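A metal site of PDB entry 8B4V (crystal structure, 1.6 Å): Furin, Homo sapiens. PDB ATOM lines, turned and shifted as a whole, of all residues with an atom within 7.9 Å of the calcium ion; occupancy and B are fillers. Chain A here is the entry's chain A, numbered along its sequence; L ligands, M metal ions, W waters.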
ATOM      1  N   GLY A 148       5.700 -12.124  -7.145  1.00  0.00           N
ATOM      2  CA  GLY A 148       4.246 -12.195  -7.188  1.00  0.00           C
ATOM      3  C   GLY A 148       3.554 -11.113  -6.361  1.00  0.00           C
ATOM      4  O   GLY A 148       4.197 -10.143  -5.934  1.00  0.00           O
ATOM      5  N   PRO A 149       2.252 -11.266  -6.083  1.00  0.00           N
ATOM      6  CA  PRO A 149       1.537 -10.244  -5.291  1.00  0.00           C
ATOM      7  C   PRO A 149       2.157 -10.047  -3.907  1.00  0.00           C
ATOM      8  O   PRO A 149       2.757 -10.962  -3.353  1.00  0.00           O
ATOM      9  CB  PRO A 149       0.115 -10.789  -5.161  1.00  0.00           C
ATOM     10  CG  PRO A 149       0.052 -12.007  -5.999  1.00  0.00           C
ATOM     11  CD  PRO A 149       1.402 -12.413  -6.438  1.00  0.00           C
ATOM     12  N   GLU A 150       1.970  -8.848  -3.362  1.00  0.00           N
ATOM     13  CA  GLU A 150       2.603  -8.484  -2.095  1.00  0.00           C
ATOM     14  C   GLU A 150       2.314  -9.532  -1.022  1.00  0.00           C
ATOM     15  O   GLU A 150       1.166  -9.928  -0.806  1.00  0.00           O
ATOM     16  CB  GLU A 150       2.113  -7.118  -1.626  1.00  0.00           C
ATOM     17  CG  GLU A 150       2.809  -6.639  -0.358  1.00  0.00           C
ATOM     18  CD  GLU A 150       2.621  -5.156  -0.084  1.00  0.00           C
ATOM     19  OE1 GLU A 150       1.833  -4.505  -0.809  1.00  0.00           O
ATOM     20  OE2 GLU A 150       3.265  -4.649   0.854  1.00  0.00           O
ATOM     21  N   ASP A 151       3.379  -9.988  -0.365  1.00  0.00           N
ATOM     22  CA  ASP A 151       3.290 -11.002   0.689  1.00  0.00           C
ATOM     23  C   ASP A 151       2.990 -10.383   2.045  1.00  0.00           C
ATOM     24  O   ASP A 151       3.637 -10.688   3.051  1.00  0.00           O
ATOM     25  CB  ASP A 151       4.594 -11.802   0.748  1.00  0.00           C
ATOM     26  CG  ASP A 151       4.772 -12.766  -0.418  1.00  0.00           C
ATOM     27  OD1 ASP A 151       3.758 -13.227  -0.981  1.00  0.00           O
ATOM     28  OD2 ASP A 151       5.948 -13.103  -0.731  1.00  0.00           O
ATOM     29  N   ASP A 152       1.988  -9.492   2.094  1.00  0.00           N
ATOM     30  CA  ASP A 152       1.643  -8.809   3.335  1.00  0.00           C
ATOM     31  C   ASP A 152       0.599  -9.559   4.149  1.00  0.00           C
ATOM     32  O   ASP A 152       0.268  -9.113   5.250  1.00  0.00           O
ATOM     33  CB  ASP A 152       1.167  -7.367   3.071  1.00  0.00           C
ATOM     34  CG  ASP A 152       0.009  -7.276   2.090  1.00  0.00           C
ATOM     35  OD1 ASP A 152      -0.587  -8.311   1.718  1.00  0.00           O
ATOM     36  OD2 ASP A 152      -0.320  -6.137   1.699  1.00  0.00           O
ATOM     37  N   GLY A 153       0.105 -10.696   3.645  1.00  0.00           N
ATOM     38  CA  GLY A 153      -0.900 -11.437   4.363  1.00  0.00           C
ATOM     39  C   GLY A 153      -2.267 -10.821   4.319  1.00  0.00           C
ATOM     40  O   GLY A 153      -3.145 -11.218   5.083  1.00  0.00           O
ATOM     41  N   LYS A 154      -2.470  -9.829   3.450  1.00  0.00           N
ATOM     42  CA  LYS A 154      -3.797  -9.256   3.300  1.00  0.00           C
ATOM     43  C   LYS A 154      -4.246  -9.106   1.854  1.00  0.00           C
ATOM     44  O   LYS A 154      -5.361  -8.639   1.626  1.00  0.00           O
ATOM     45  CB  LYS A 154      -3.895  -7.887   3.994  1.00  0.00           C
ATOM     46  CG  LYS A 154      -2.729  -6.949   3.810  1.00  0.00           C
ATOM     47  CD  LYS A 154      -2.913  -5.745   4.758  1.00  0.00           C
ATOM     48  CE  LYS A 154      -1.775  -4.756   4.664  1.00  0.00           C
ATOM     49  N   THR A 155      -3.425  -9.507   0.896  1.00  0.00           N
ATOM     50  CA  THR A 155      -3.712  -9.314  -0.520  1.00  0.00           C
ATOM     51  C   THR A 155      -4.283 -10.589  -1.124  1.00  0.00           C
ATOM     52  O   THR A 155      -3.833 -11.699  -0.794  1.00  0.00           O
ATOM     53  CB  THR A 155      -2.427  -8.893  -1.228  1.00  0.00           C
ATOM     54  OG1 THR A 155      -1.938  -7.673  -0.645  1.00  0.00           O
ATOM     55  CG2 THR A 155      -2.654  -8.675  -2.713  1.00  0.00           C
ATOM     56  N   ALA A 185       7.895 -19.652  -7.323  1.00  0.00           N
ATOM     57  CA  ALA A 185       8.128 -19.641  -5.881  1.00  0.00           C
ATOM     58  C   ALA A 185       6.802 -19.388  -5.162  1.00  0.00           C
ATOM     59  O   ALA A 185       6.077 -18.459  -5.513  1.00  0.00           O
ATOM     60  CB  ALA A 185       9.124 -18.545  -5.498  1.00  0.00           C
ATOM     61  N   SER A 186       6.507 -20.180  -4.129  1.00  0.00           N
ATOM     62  CA  SER A 186       5.169 -20.098  -3.549  1.00  0.00           C
ATOM     63  C   SER A 186       4.938 -18.883  -2.657  1.00  0.00           C
ATOM     64  O   SER A 186       3.773 -18.611  -2.325  1.00  0.00           O
ATOM     65  CB  SER A 186       4.830 -21.367  -2.754  1.00  0.00           C
ATOM     66  OG  SER A 186       5.739 -21.570  -1.674  1.00  0.00           O
ATOM     67  N   GLY A 187       5.970 -18.173  -2.235  1.00  0.00           N
ATOM     68  CA  GLY A 187       5.786 -16.966  -1.452  1.00  0.00           C
ATOM     69  C   GLY A 187       6.711 -16.861  -0.254  1.00  0.00           C
ATOM     70  O   GLY A 187       7.213 -17.849   0.283  1.00  0.00           O
ATOM     71  N   ASN A 188       6.946 -15.618   0.188  1.00  0.00           N
ATOM     72  CA  ASN A 188       7.816 -15.341   1.323  1.00  0.00           C
ATOM     73  C   ASN A 188       7.083 -14.657   2.474  1.00  0.00           C
ATOM     74  O   ASN A 188       7.717 -13.983   3.301  1.00  0.00           O
ATOM     75  CB  ASN A 188       9.007 -14.477   0.901  1.00  0.00           C
ATOM     76  CG  ASN A 188       9.999 -15.226   0.047  1.00  0.00           C
ATOM     77  OD1 ASN A 188      10.207 -16.418   0.226  1.00  0.00           O
ATOM     78  ND2 ASN A 188      10.628 -14.525  -0.892  1.00  0.00           N
ATOM     79  N   GLY A 189       5.770 -14.854   2.577  1.00  0.00           N
ATOM     80  CA  GLY A 189       4.952 -14.133   3.540  1.00  0.00           C
ATOM     81  C   GLY A 189       4.707 -14.797   4.884  1.00  0.00           C
ATOM     82  O   GLY A 189       3.762 -14.423   5.594  1.00  0.00           O
ATOM     83  N   GLY A 190       5.562 -15.741   5.268  1.00  0.00           N
ATOM     84  CA  GLY A 190       5.336 -16.480   6.506  1.00  0.00           C
ATOM     85  C   GLY A 190       5.232 -15.605   7.746  1.00  0.00           C
ATOM     86  O   GLY A 190       4.443 -15.886   8.648  1.00  0.00           O
ATOM     87  N   HIS A 193       1.889 -14.455   8.274  1.00  0.00           N
ATOM     88  CA  HIS A 193       0.924 -15.555   8.223  1.00  0.00           C
ATOM     89  C   HIS A 193       0.140 -15.570   6.907  1.00  0.00           C
ATOM     90  O   HIS A 193      -1.058 -15.851   6.883  1.00  0.00           O
ATOM     91  CB  HIS A 193      -0.025 -15.512   9.430  1.00  0.00           C
ATOM     92  CG  HIS A 193       0.650 -15.775  10.746  1.00  0.00           C
ATOM     93  ND1 HIS A 193       0.094 -16.572  11.725  1.00  0.00           N
ATOM     94  CD2 HIS A 193       1.845 -15.367  11.228  1.00  0.00           C
ATOM     95  CE1 HIS A 193       0.912 -16.630  12.752  1.00  0.00           C
ATOM     96  NE2 HIS A 193       1.985 -15.907  12.482  1.00  0.00           N
ATOM     97  N   ASP A 194       0.833 -15.300   5.805  1.00  0.00           N
ATOM     98  CA  ASP A 194       0.204 -15.347   4.492  1.00  0.00           C
ATOM     99  C   ASP A 194      -0.111 -16.797   4.099  1.00  0.00           C
ATOM    100  O   ASP A 194       0.519 -17.741   4.568  1.00  0.00           O
ATOM    101  CB  ASP A 194       1.116 -14.674   3.460  1.00  0.00           C
ATOM    102  CG  ASP A 194       0.389 -14.180   2.216  1.00  0.00           C
ATOM    103  OD1 ASP A 194      -0.853 -14.317   2.124  1.00  0.00           O
ATOM    104  OD2 ASP A 194       1.076 -13.668   1.307  1.00  0.00           O
ATOM    105  N   SER A 195      -1.097 -16.943   3.214  1.00  0.00           N
ATOM    106  CA  SER A 195      -1.673 -18.229   2.813  1.00  0.00           C
ATOM    107  C   SER A 195      -1.631 -18.195   1.281  1.00  0.00           C
ATOM    108  O   SER A 195      -2.279 -17.346   0.666  1.00  0.00           O
ATOM    109  CB  SER A 195      -3.085 -18.362   3.369  1.00  0.00           C
ATOM    110  OG  SER A 195      -3.633 -19.677   3.305  1.00  0.00           O
ATOM    111  N   CYS A 196      -0.828 -19.085   0.662  1.00  0.00           N
ATOM    112  CA  CYS A 196      -0.409 -18.814  -0.711  1.00  0.00           C
ATOM    113  C   CYS A 196      -1.459 -19.148  -1.766  1.00  0.00           C
ATOM    114  O   CYS A 196      -1.222 -18.854  -2.941  1.00  0.00           O
ATOM    115  CB  CYS A 196       0.922 -19.531  -1.042  1.00  0.00           C
ATOM    116  SG  CYS A 196       1.279 -21.183  -0.384  1.00  0.00           S
ATOM    117  N   ASN A 197      -2.623 -19.715  -1.413  1.00  0.00           N
ATOM    118  CA  ASN A 197      -3.660 -19.796  -2.435  1.00  0.00           C
ATOM    119  C   ASN A 197      -4.264 -18.426  -2.740  1.00  0.00           C
ATOM    120  O   ASN A 197      -5.010 -18.301  -3.714  1.00  0.00           O
ATOM    121  CB  ASN A 197      -4.806 -20.736  -2.033  1.00  0.00           C
ATOM    122  CG  ASN A 197      -4.413 -22.201  -2.062  1.00  0.00           C
ATOM    123  OD1 ASN A 197      -3.388 -22.608  -2.625  1.00  0.00           O
ATOM    124  ND2 ASN A 197      -5.263 -23.022  -1.465  1.00  0.00           N
ATOM    125  N   CYS A 198      -3.940 -17.396  -1.951  1.00  0.00           N
ATOM    126  CA  CYS A 198      -4.362 -16.029  -2.224  1.00  0.00           C
ATOM    127  C   CYS A 198      -3.488 -15.318  -3.253  1.00  0.00           C
ATOM    128  O   CYS A 198      -3.717 -14.132  -3.529  1.00  0.00           O
ATOM    129  CB  CYS A 198      -4.400 -15.211  -0.926  1.00  0.00           C
ATOM    130  SG  CYS A 198      -5.651 -15.745   0.256  1.00  0.00           S
ATOM    131  N   ASP A 199      -2.514 -16.032  -3.824  1.00  0.00           N
ATOM    132  CA  ASP A 199      -1.602 -15.578  -4.860  1.00  0.00           C
ATOM    133  C   ASP A 199      -1.969 -16.369  -6.110  1.00  0.00           C
ATOM    134  O   ASP A 199      -1.726 -17.574  -6.176  1.00  0.00           O
ATOM    135  CB  ASP A 199      -0.177 -15.811  -4.359  1.00  0.00           C
ATOM    136  CG  ASP A 199       0.894 -15.660  -5.417  1.00  0.00           C
ATOM    137  OD1 ASP A 199       0.592 -15.669  -6.631  1.00  0.00           O
ATOM    138  OD2 ASP A 199       2.072 -15.555  -5.011  1.00  0.00           O
ATOM    139  N   THR A 202       0.942 -18.485  -8.078  1.00  0.00           N
ATOM    140  CA  THR A 202       1.306 -19.804  -7.565  1.00  0.00           C
ATOM    141  C   THR A 202       0.094 -20.732  -7.499  1.00  0.00           C
ATOM    142  O   THR A 202       0.248 -21.942  -7.710  1.00  0.00           O
ATOM    143  CB  THR A 202       1.993 -19.650  -6.212  1.00  0.00           C
ATOM    144  OG1 THR A 202       2.634 -20.889  -5.864  1.00  0.00           O
ATOM    145  CG2 THR A 202       1.027 -19.183  -5.156  1.00  0.00           C
ATOM    146  N   TYR A 222       9.793 -17.843   6.618  1.00  0.00           N
ATOM    147  CA  TYR A 222       9.150 -17.097   5.540  1.00  0.00           C
ATOM    148  C   TYR A 222       8.132 -17.933   4.765  1.00  0.00           C
ATOM    149  O   TYR A 222       7.459 -17.404   3.875  1.00  0.00           O
ATOM    150  CB  TYR A 222      10.209 -16.543   4.554  1.00  0.00           C
ATOM    151  CG  TYR A 222      11.196 -17.600   4.108  1.00  0.00           C
ATOM    152  CD1 TYR A 222      10.851 -18.533   3.130  1.00  0.00           C
ATOM    153  CD2 TYR A 222      12.441 -17.704   4.696  1.00  0.00           C
ATOM    154  CE1 TYR A 222      11.728 -19.515   2.748  1.00  0.00           C
ATOM    155  CE2 TYR A 222      13.334 -18.702   4.322  1.00  0.00           C
ATOM    156  CZ  TYR A 222      12.964 -19.603   3.348  1.00  0.00           C
ATOM    157  OH  TYR A 222      13.819 -20.603   2.949  1.00  0.00           O
ATOM    158  N   GLU A 224       4.976 -19.946   3.291  1.00  0.00           N
ATOM    159  CA  GLU A 224       3.521 -19.927   3.236  1.00  0.00           C
ATOM    160  C   GLU A 224       3.025 -21.339   2.952  1.00  0.00           C
ATOM    161  O   GLU A 224       3.490 -21.984   2.012  1.00  0.00           O
ATOM    162  CB  GLU A 224       3.021 -18.986   2.154  1.00  0.00           C
ATOM    163  CG  GLU A 224       3.459 -17.539   2.335  1.00  0.00           C
ATOM    164  CD  GLU A 224       2.950 -16.600   1.242  1.00  0.00           C
ATOM    165  OE1 GLU A 224       3.727 -15.697   0.838  1.00  0.00           O
ATOM    166  OE2 GLU A 224       1.783 -16.717   0.803  1.00  0.00           O
ATOM    167  N   ARG A 412      -5.958 -15.498   8.090  1.00  0.00           N
ATOM    168  CA  ARG A 412      -4.922 -14.495   7.832  1.00  0.00           C
ATOM    169  C   ARG A 412      -5.169 -13.314   8.756  1.00  0.00           C
ATOM    170  O   ARG A 412      -6.051 -12.477   8.490  1.00  0.00           O
ATOM    171  CB  ARG A 412      -4.931 -14.065   6.366  1.00  0.00           C
ATOM    172  CG  ARG A 412      -4.431 -15.157   5.430  1.00  0.00           C
ATOM    173  CD  ARG A 412      -3.922 -14.633   4.090  1.00  0.00           C
ATOM    174  NE  ARG A 412      -4.908 -13.807   3.397  1.00  0.00           N
ATOM    175  CZ  ARG A 412      -4.631 -13.043   2.346  1.00  0.00           C
ATOM    176  NH1 ARG A 412      -5.584 -12.291   1.796  1.00  0.00           N
ATOM    177  NH2 ARG A 412      -3.408 -13.023   1.855  1.00  0.00           N
HETATM  178  C1  LIG L   1       6.501 -14.351  -4.152  1.00  0.00           C
HETATM  179  C2  LIG L   1       6.887 -13.038  -3.883  1.00  0.00           C
HETATM  180  C3  LIG L   1       8.220 -12.724  -3.619  1.00  0.00           C
HETATM  181  C4  LIG L   1       9.179 -13.730  -3.615  1.00  0.00           C
HETATM  182  C5  LIG L   1       8.816 -15.044  -3.882  1.00  0.00           C
HETATM  183  C6  LIG L   1       7.479 -15.349  -4.144  1.00  0.00           C
HETATM  184  C7  LIG L   1       5.156 -14.657  -4.426  1.00  0.00           C
HETATM  185  N1  LIG L   1       4.205 -13.796  -4.038  1.00  0.00           N
HETATM  186  N2  LIG L   1       4.869 -15.790  -5.089  1.00  0.00           N
HETATM  187 CA    CA M   1       1.956 -14.726  -0.572  1.00  0.00          CA
HETATM  188  O   HOH W   1      -0.431 -15.176  -0.832  1.00  0.00           O
HETATM  189  O   HOH W   2       2.430 -16.251  -2.343  1.00  0.00           O
HETATM  190  O   HOH W   3       1.134 -13.079  -2.144  1.00  0.00           O
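O of Pro 149 sits at hydrogen-bond distance from N1 of the ligand (3.3 Å). A nitrogen (N2) of the ligand sits at hydrogen-bond distance from the backbone carbonyl oxygen of Ala 185, 3.0 Å away. A nitrogen (N1) of the ligand is in salt-bridge range of the side-chain carboxylate of Asp 151 (3.8 Å). OD2 of Asp 199 lies within salt-bridge range of N2 of the ligand (2.8 Å).
The calcium ion is bound by the side-chain carboxylate (OD2) of Asp 194 (2.3 Å), the side-chain carboxylate (OD1) of Asp 151 (2.4 Å), water W2 (2.4 Å), water W3 (2.4 Å), the side-chain carboxylate (OE2) of Glu 224 (2.4 Å), water W1 (2.4 Å) and the side-chain carboxylate (OE1) of Glu 224 (2.5 Å). The calcium ion has seven donor atoms within binding distance.
Three residues have an atom within 4 Å of the calcium ion: Asp 151, Asp 194 and Glu 224.
OD1 of Asp 194 lies within salt-bridge range of NH2 of Arg 412 (2.9 Å). The side-chain carboxylate of Glu 224 lies close to the backbone NH of Gly 189. The side-chain carboxylate (OD2) of Asp 151 sits at hydrogen-bond distance from the backbone NH (N) of Asn 188. N of Asp 194 is in hydrogen-bond range of O of Gly 189 (3.1 Å). The backbone NH (N) of Asn 188 lies close to the side-chain carboxylate (OE1) of Glu 224, at 3.3 Å.
Water W2 lies within hydrogen-bond range of the backbone carbonyl oxygen (O) of Ser 186 (2.7 Å), the side-chain carboxylate (OD2) of Asp 199 (2.8 Å) and a nitrogen (N1) of the ligand (3.5 Å). Water W1 bridges OD1 of Asp 194 (3.1 Å) and O of Ser 195 (3.2 Å).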
